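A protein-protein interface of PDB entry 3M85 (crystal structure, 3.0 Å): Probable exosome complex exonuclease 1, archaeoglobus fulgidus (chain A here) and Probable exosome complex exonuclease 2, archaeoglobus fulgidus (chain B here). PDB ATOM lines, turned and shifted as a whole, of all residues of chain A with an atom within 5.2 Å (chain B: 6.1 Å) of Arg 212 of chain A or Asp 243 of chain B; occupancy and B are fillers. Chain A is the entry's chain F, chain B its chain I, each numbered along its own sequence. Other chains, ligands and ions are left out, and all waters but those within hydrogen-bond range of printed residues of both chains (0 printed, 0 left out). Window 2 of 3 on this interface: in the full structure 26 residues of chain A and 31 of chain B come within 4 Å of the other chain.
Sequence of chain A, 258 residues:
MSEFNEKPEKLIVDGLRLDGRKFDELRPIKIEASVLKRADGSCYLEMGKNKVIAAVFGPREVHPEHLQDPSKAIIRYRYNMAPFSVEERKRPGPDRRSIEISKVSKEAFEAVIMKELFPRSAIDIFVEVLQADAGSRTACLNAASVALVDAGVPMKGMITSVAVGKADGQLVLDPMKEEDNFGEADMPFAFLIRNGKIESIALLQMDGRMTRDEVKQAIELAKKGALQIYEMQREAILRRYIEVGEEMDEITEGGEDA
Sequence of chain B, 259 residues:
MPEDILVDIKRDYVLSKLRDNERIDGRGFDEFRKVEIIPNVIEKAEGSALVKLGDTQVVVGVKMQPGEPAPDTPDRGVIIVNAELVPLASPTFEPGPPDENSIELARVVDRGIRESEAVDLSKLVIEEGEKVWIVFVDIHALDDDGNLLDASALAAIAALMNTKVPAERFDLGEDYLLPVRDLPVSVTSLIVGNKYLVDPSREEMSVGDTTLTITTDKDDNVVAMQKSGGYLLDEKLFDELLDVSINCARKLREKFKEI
Of the 15 printed residues of chain B, 7 touch a printed residue of chain A. Hydrophobic or aromatic side chains of chain A that line the printed part of chain B: Val 215. Among the printed residues, 9 pairs touch across the chains. Among the printed residues, Asp or Glu carboxylates within 4 Å of a Lys or Arg side-chain nitrogen of the other chain: Arg 212 of chain A with Asp 243 of chain B (3.0 Å).
Asn 221 of chain B touches Met 210 of chain A. Thr 211 of chain A touches Asn 221 of chain B (CG2 to OD1, 3.9 Å). Arg 212 of chain A touches Leu 242 of chain B (CG to CD1, 3.5 Å). Arg 212 of chain A touches Ile 246 of chain B. Val 215 of chain A touches Phe 238 of chain B (CG1 to CE2, 3.7 Å). Asp 239 of chain B touches Lys 216 of chain A. CG of Lys 216 of chain A touches CD1 of Leu 242 of chain B, at 3.8 Å.
Of the printed residues of chain B, Thr 211 of chain A touches Asn 221 (3.9 Å). Arg 212 of chain A touches just these residues of chain B: Leu 242, Asp 243 and Ile 246. Printed residues of chain A within 4 Å of Asn 221 of chain B: Met 210 and Thr 211. Asp 243 of chain B touches just one residue of chain A: Arg 212 (3.0 Å). Printed residues of chain A within 4 Å of Ile 246 of chain B: Arg 212 (3.5 Å). The nearest residue of chain B that does not touch Arg 212 of chain A is Val 222 of chain B (4.7 Å). The nearest printed residue of chain A that does not touch Leu 242 of chain B is Val 215 of chain A (4.03 Å).
OE1 of Glu 214 of chain A lies within hydrogen-bond range of N of Thr 211 of chain A (3.0 Å). The side-chain carboxylate of Asp 213 of chain A lies within salt-bridge range of the guanidinium group of Arg 212 of chain A.
The backbone NH of Val 222 of chain B is in hydrogen-bond range of the backbone carbonyl oxygen of Met 210 of chain A, 2.6 Å away. The side-chain carboxylate (OD2) of Asp 243 of chain B is in salt-bridge range of the guanidinium group (NH1) of Arg 212 of chain A (3.0 Å).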
ATOM      1  N   MET A 210      14.168  24.628 -21.059  1.00  0.00           N
ATOM      2  CA  MET A 210      14.340  25.831 -21.869  1.00  0.00           C
ATOM      3  C   MET A 210      14.633  25.492 -23.346  1.00  0.00           C
ATOM      4  O   MET A 210      15.239  24.453 -23.680  1.00  0.00           O
ATOM      5  CB  MET A 210      15.473  26.720 -21.343  1.00  0.00           C
ATOM      6  CG  MET A 210      15.443  27.123 -19.881  1.00  0.00           C
ATOM      7  SD  MET A 210      16.922  28.122 -19.425  1.00  0.00           S
ATOM      8  CE  MET A 210      16.460  29.738 -20.029  1.00  0.00           C
ATOM      9  N   THR A 211      14.212  26.392 -24.225  1.00  0.00           N
ATOM     10  CA  THR A 211      14.551  26.309 -25.632  1.00  0.00           C
ATOM     11  C   THR A 211      15.964  26.791 -25.842  1.00  0.00           C
ATOM     12  O   THR A 211      16.454  27.641 -25.113  1.00  0.00           O
ATOM     13  CB  THR A 211      13.627  27.176 -26.473  1.00  0.00           C
ATOM     14  OG1 THR A 211      13.812  28.559 -26.127  1.00  0.00           O
ATOM     15  CG2 THR A 211      12.190  26.768 -26.255  1.00  0.00           C
ATOM     16  N   ARG A 212      16.620  26.248 -26.851  1.00  0.00           N
ATOM     17  CA  ARG A 212      18.010  26.594 -27.116  1.00  0.00           C
ATOM     18  C   ARG A 212      18.170  28.110 -27.195  1.00  0.00           C
ATOM     19  O   ARG A 212      19.187  28.674 -26.758  1.00  0.00           O
ATOM     20  CB  ARG A 212      18.460  25.901 -28.399  1.00  0.00           C
ATOM     21  CG  ARG A 212      19.744  26.387 -28.990  1.00  0.00           C
ATOM     22  CD  ARG A 212      19.474  27.352 -30.106  1.00  0.00           C
ATOM     23  NE  ARG A 212      20.679  27.635 -30.867  1.00  0.00           N
ATOM     24  CZ  ARG A 212      20.880  28.761 -31.543  1.00  0.00           C
ATOM     25  NH1 ARG A 212      22.019  28.938 -32.215  1.00  0.00           N
ATOM     26  NH2 ARG A 212      19.944  29.714 -31.539  1.00  0.00           N
ATOM     27  N   ASP A 213      17.138  28.762 -27.724  1.00  0.00           N
ATOM     28  CA  ASP A 213      17.076  30.220 -27.748  1.00  0.00           C
ATOM     29  C   ASP A 213      17.099  30.820 -26.344  1.00  0.00           C
ATOM     30  O   ASP A 213      17.842  31.760 -26.077  1.00  0.00           O
ATOM     31  CB  ASP A 213      15.805  30.682 -28.459  1.00  0.00           C
ATOM     32  CG  ASP A 213      15.955  30.743 -29.966  1.00  0.00           C
ATOM     33  OD1 ASP A 213      17.092  30.597 -30.470  1.00  0.00           O
ATOM     34  OD2 ASP A 213      14.927  30.953 -30.652  1.00  0.00           O
ATOM     35  N   GLU A 214      16.274  30.278 -25.454  1.00  0.00           N
ATOM     36  CA  GLU A 214      16.208  30.776 -24.073  1.00  0.00           C
ATOM     37  C   GLU A 214      17.538  30.623 -23.328  1.00  0.00           C
ATOM     38  O   GLU A 214      17.936  31.530 -22.600  1.00  0.00           O
ATOM     39  CB  GLU A 214      15.033  30.159 -23.289  1.00  0.00           C
ATOM     40  CG  GLU A 214      13.695  30.783 -23.629  1.00  0.00           C
ATOM     41  CD  GLU A 214      12.467  29.909 -23.328  1.00  0.00           C
ATOM     42  OE1 GLU A 214      12.585  28.676 -23.096  1.00  0.00           O
ATOM     43  OE2 GLU A 214      11.351  30.485 -23.339  1.00  0.00           O
ATOM     44  N   VAL A 215      18.238  29.504 -23.519  1.00  0.00           N
ATOM     45  CA  VAL A 215      19.576  29.365 -22.918  1.00  0.00           C
ATOM     46  C   VAL A 215      20.418  30.585 -23.287  1.00  0.00           C
ATOM     47  O   VAL A 215      20.902  31.316 -22.408  1.00  0.00           O
ATOM     48  CB  VAL A 215      20.337  28.058 -23.347  1.00  0.00           C
ATOM     49  CG1 VAL A 215      21.821  28.159 -23.020  1.00  0.00           C
ATOM     50  CG2 VAL A 215      19.742  26.826 -22.686  1.00  0.00           C
ATOM     51  N   LYS A 216      20.554  30.814 -24.595  1.00  0.00           N
ATOM     52  CA  LYS A 216      21.389  31.891 -25.103  1.00  0.00           C
ATOM     53  C   LYS A 216      20.906  33.241 -24.609  1.00  0.00           C
ATOM     54  O   LYS A 216      21.694  34.137 -24.307  1.00  0.00           O
ATOM     55  CB  LYS A 216      21.440  31.858 -26.625  1.00  0.00           C
ATOM     56  CG  LYS A 216      22.030  30.571 -27.189  1.00  0.00           C
ATOM     57  CD  LYS A 216      22.272  30.668 -28.687  1.00  0.00           C
ATOM     58  CE  LYS A 216      23.292  31.754 -29.017  1.00  0.00           C
ATOM     59  NZ  LYS A 216      23.687  31.717 -30.462  1.00  0.00           N
ATOM     60  N   ILE B 214      25.276  18.574 -21.476  1.00  0.00           N
ATOM     61  CA  ILE B 214      23.988  19.142 -21.813  1.00  0.00           C
ATOM     62  C   ILE B 214      22.984  18.001 -22.058  1.00  0.00           C
ATOM     63  O   ILE B 214      23.274  17.054 -22.801  1.00  0.00           O
ATOM     64  CB  ILE B 214      24.127  19.996 -23.047  1.00  0.00           C
ATOM     65  CG1 ILE B 214      25.122  21.113 -22.785  1.00  0.00           C
ATOM     66  CG2 ILE B 214      22.789  20.531 -23.497  1.00  0.00           C
ATOM     67  CD1 ILE B 214      25.207  22.076 -23.916  1.00  0.00           C
ATOM     68  N   ASP B 220      13.791  18.633 -28.217  1.00  0.00           N
ATOM     69  CA  ASP B 220      15.015  19.435 -28.330  1.00  0.00           C
ATOM     70  C   ASP B 220      15.118  20.628 -27.367  1.00  0.00           C
ATOM     71  O   ASP B 220      15.891  21.569 -27.601  1.00  0.00           O
ATOM     72  CB  ASP B 220      15.239  19.877 -29.771  1.00  0.00           C
ATOM     73  CG  ASP B 220      15.675  18.728 -30.661  1.00  0.00           C
ATOM     74  OD1 ASP B 220      16.385  17.822 -30.156  1.00  0.00           O
ATOM     75  OD2 ASP B 220      15.301  18.726 -31.856  1.00  0.00           O
ATOM     76  N   ASN B 221      14.328  20.590 -26.296  1.00  0.00           N
ATOM     77  CA  ASN B 221      14.475  21.532 -25.214  1.00  0.00           C
ATOM     78  C   ASN B 221      15.694  21.162 -24.422  1.00  0.00           C
ATOM     79  O   ASN B 221      15.958  19.976 -24.227  1.00  0.00           O
ATOM     80  CB  ASN B 221      13.275  21.445 -24.298  1.00  0.00           C
ATOM     81  CG  ASN B 221      12.026  21.966 -24.939  1.00  0.00           C
ATOM     82  OD1 ASN B 221      12.060  22.908 -25.729  1.00  0.00           O
ATOM     83  ND2 ASN B 221      10.898  21.357 -24.596  1.00  0.00           N
ATOM     84  N   VAL B 222      16.440  22.161 -23.958  1.00  0.00           N
ATOM     85  CA  VAL B 222      17.496  21.899 -22.994  1.00  0.00           C
ATOM     86  C   VAL B 222      16.852  21.728 -21.620  1.00  0.00           C
ATOM     87  O   VAL B 222      16.007  22.525 -21.204  1.00  0.00           O
ATOM     88  CB  VAL B 222      18.494  23.031 -22.940  1.00  0.00           C
ATOM     89  CG1 VAL B 222      19.444  22.827 -21.775  1.00  0.00           C
ATOM     90  CG2 VAL B 222      19.262  23.111 -24.242  1.00  0.00           C
ATOM     91  N   PHE B 238      30.866  27.931 -25.490  1.00  0.00           N
ATOM     92  CA  PHE B 238      29.676  27.326 -24.946  1.00  0.00           C
ATOM     93  C   PHE B 238      28.535  27.385 -25.957  1.00  0.00           C
ATOM     94  O   PHE B 238      27.790  26.409 -26.142  1.00  0.00           O
ATOM     95  CB  PHE B 238      29.231  27.948 -23.628  1.00  0.00           C
ATOM     96  CG  PHE B 238      27.858  27.510 -23.232  1.00  0.00           C
ATOM     97  CD1 PHE B 238      27.647  26.232 -22.745  1.00  0.00           C
ATOM     98  CD2 PHE B 238      26.762  28.342 -23.434  1.00  0.00           C
ATOM     99  CE1 PHE B 238      26.382  25.810 -22.430  1.00  0.00           C
ATOM    100  CE2 PHE B 238      25.482  27.916 -23.115  1.00  0.00           C
ATOM    101  CZ  PHE B 238      25.292  26.652 -22.615  1.00  0.00           C
ATOM    102  N   ASP B 239      28.401  28.540 -26.601  1.00  0.00           N
ATOM    103  CA  ASP B 239      27.299  28.768 -27.532  1.00  0.00           C
ATOM    104  C   ASP B 239      27.316  27.734 -28.647  1.00  0.00           C
ATOM    105  O   ASP B 239      26.290  27.167 -29.025  1.00  0.00           O
ATOM    106  CB  ASP B 239      27.369  30.175 -28.133  1.00  0.00           C
ATOM    107  CG  ASP B 239      26.605  31.214 -27.309  1.00  0.00           C
ATOM    108  OD1 ASP B 239      25.782  30.838 -26.437  1.00  0.00           O
ATOM    109  OD2 ASP B 239      26.824  32.424 -27.543  1.00  0.00           O
ATOM    110  N   GLU B 240      28.498  27.484 -29.162  1.00  0.00           N
ATOM    111  CA  GLU B 240      28.627  26.599 -30.293  1.00  0.00           C
ATOM    112  C   GLU B 240      28.448  25.122 -29.908  1.00  0.00           C
ATOM    113  O   GLU B 240      27.855  24.336 -30.643  1.00  0.00           O
ATOM    114  CB  GLU B 240      29.946  26.905 -31.010  1.00  0.00           C
ATOM    115  CG  GLU B 240      30.757  25.750 -31.530  1.00  0.00           C
ATOM    116  CD  GLU B 240      31.968  26.287 -32.251  1.00  0.00           C
ATOM    117  OE1 GLU B 240      32.846  25.486 -32.678  1.00  0.00           O
ATOM    118  OE2 GLU B 240      32.022  27.539 -32.382  1.00  0.00           O
ATOM    119  N   LEU B 241      28.935  24.759 -28.739  1.00  0.00           N
ATOM    120  CA  LEU B 241      28.786  23.404 -28.241  1.00  0.00           C
ATOM    121  C   LEU B 241      27.339  23.100 -27.766  1.00  0.00           C
ATOM    122  O   LEU B 241      26.964  21.935 -27.554  1.00  0.00           O
ATOM    123  CB  LEU B 241      29.804  23.205 -27.122  1.00  0.00           C
ATOM    124  CG  LEU B 241      29.894  21.856 -26.437  1.00  0.00           C
ATOM    125  CD1 LEU B 241      29.837  20.736 -27.456  1.00  0.00           C
ATOM    126  CD2 LEU B 241      31.191  21.831 -25.650  1.00  0.00           C
ATOM    127  N   LEU B 242      26.543  24.160 -27.603  1.00  0.00           N
ATOM    128  CA  LEU B 242      25.140  24.037 -27.247  1.00  0.00           C
ATOM    129  C   LEU B 242      24.435  23.325 -28.370  1.00  0.00           C
ATOM    130  O   LEU B 242      23.677  22.377 -28.158  1.00  0.00           O
ATOM    131  CB  LEU B 242      24.513  25.428 -27.113  1.00  0.00           C
ATOM    132  CG  LEU B 242      23.286  25.712 -26.210  1.00  0.00           C
ATOM    133  CD1 LEU B 242      22.412  26.831 -26.780  1.00  0.00           C
ATOM    134  CD2 LEU B 242      22.443  24.478 -25.907  1.00  0.00           C
ATOM    135  N   ASP B 243      24.692  23.806 -29.578  1.00  0.00           N
ATOM    136  CA  ASP B 243      24.019  23.323 -30.774  1.00  0.00           C
ATOM    137  C   ASP B 243      24.477  21.940 -31.210  1.00  0.00           C
ATOM    138  O   ASP B 243      23.672  21.088 -31.570  1.00  0.00           O
ATOM    139  CB  ASP B 243      24.232  24.314 -31.897  1.00  0.00           C
ATOM    140  CG  ASP B 243      23.276  25.468 -31.829  1.00  0.00           C
ATOM    141  OD1 ASP B 243      22.064  25.231 -32.103  1.00  0.00           O
ATOM    142  OD2 ASP B 243      23.733  26.599 -31.513  1.00  0.00           O
ATOM    143  N   VAL B 244      25.780  21.720 -31.190  1.00  0.00           N
ATOM    144  CA  VAL B 244      26.322  20.409 -31.485  1.00  0.00           C
ATOM    145  C   VAL B 244      25.723  19.368 -30.546  1.00  0.00           C
ATOM    146  O   VAL B 244      25.389  18.254 -30.969  1.00  0.00           O
ATOM    147  CB  VAL B 244      27.834  20.406 -31.305  1.00  0.00           C
ATOM    148  CG1 VAL B 244      28.367  19.000 -31.338  1.00  0.00           C
ATOM    149  CG2 VAL B 244      28.471  21.276 -32.349  1.00  0.00           C
ATOM    150  N   SER B 245      25.578  19.729 -29.273  1.00  0.00           N
ATOM    151  CA  SER B 245      25.092  18.775 -28.293  1.00  0.00           C
ATOM    152  C   SER B 245      23.609  18.454 -28.479  1.00  0.00           C
ATOM    153  O   SER B 245      23.194  17.289 -28.406  1.00  0.00           O
ATOM    154  CB  SER B 245      25.387  19.259 -26.869  1.00  0.00           C
ATOM    155  OG  SER B 245      26.779  19.239 -26.573  1.00  0.00           O
ATOM    156  N   ILE B 246      22.796  19.471 -28.715  1.00  0.00           N
ATOM    157  CA  ILE B 246      21.381  19.189 -28.875  1.00  0.00           C
ATOM    158  C   ILE B 246      21.260  18.204 -30.037  1.00  0.00           C
ATOM    159  O   ILE B 246      20.556  17.191 -29.955  1.00  0.00           O
ATOM    160  CB  ILE B 246      20.568  20.467 -29.135  1.00  0.00           C
ATOM    161  CG1 ILE B 246      20.812  21.470 -28.009  1.00  0.00           C
ATOM    162  CG2 ILE B 246      19.074  20.152 -29.305  1.00  0.00           C
ATOM    163  CD1 ILE B 246      20.095  22.786 -28.188  1.00  0.00           C
ATOM    164  N   ASN B 247      21.997  18.496 -31.100  1.00  0.00           N
ATOM    165  CA  ASN B 247      22.039  17.653 -32.282  1.00  0.00           C
ATOM    166  C   ASN B 247      22.428  16.213 -31.995  1.00  0.00           C
ATOM    167  O   ASN B 247      21.709  15.299 -32.380  1.00  0.00           O
ATOM    168  CB  ASN B 247      23.031  18.235 -33.264  1.00  0.00           C
ATOM    169  CG  ASN B 247      22.615  18.028 -34.684  1.00  0.00           C
ATOM    170  OD1 ASN B 247      22.614  16.904 -35.181  1.00  0.00           O
ATOM    171  ND2 ASN B 247      22.251  19.121 -35.356  1.00  0.00           N
ATOM    172  N   CYS B 248      23.565  16.020 -31.326  1.00  0.00           N
ATOM    173  CA  CYS B 248      24.022  14.689 -30.941  1.00  0.00           C
ATOM    174  C   CYS B 248      22.937  13.944 -30.178  1.00  0.00           C
ATOM    175  O   CYS B 248      22.736  12.733 -30.338  1.00  0.00           O
ATOM    176  CB  CYS B 248      25.271  14.776 -30.069  1.00  0.00           C
ATOM    177  SG  CYS B 248      26.812  15.312 -30.904  1.00  0.00           S
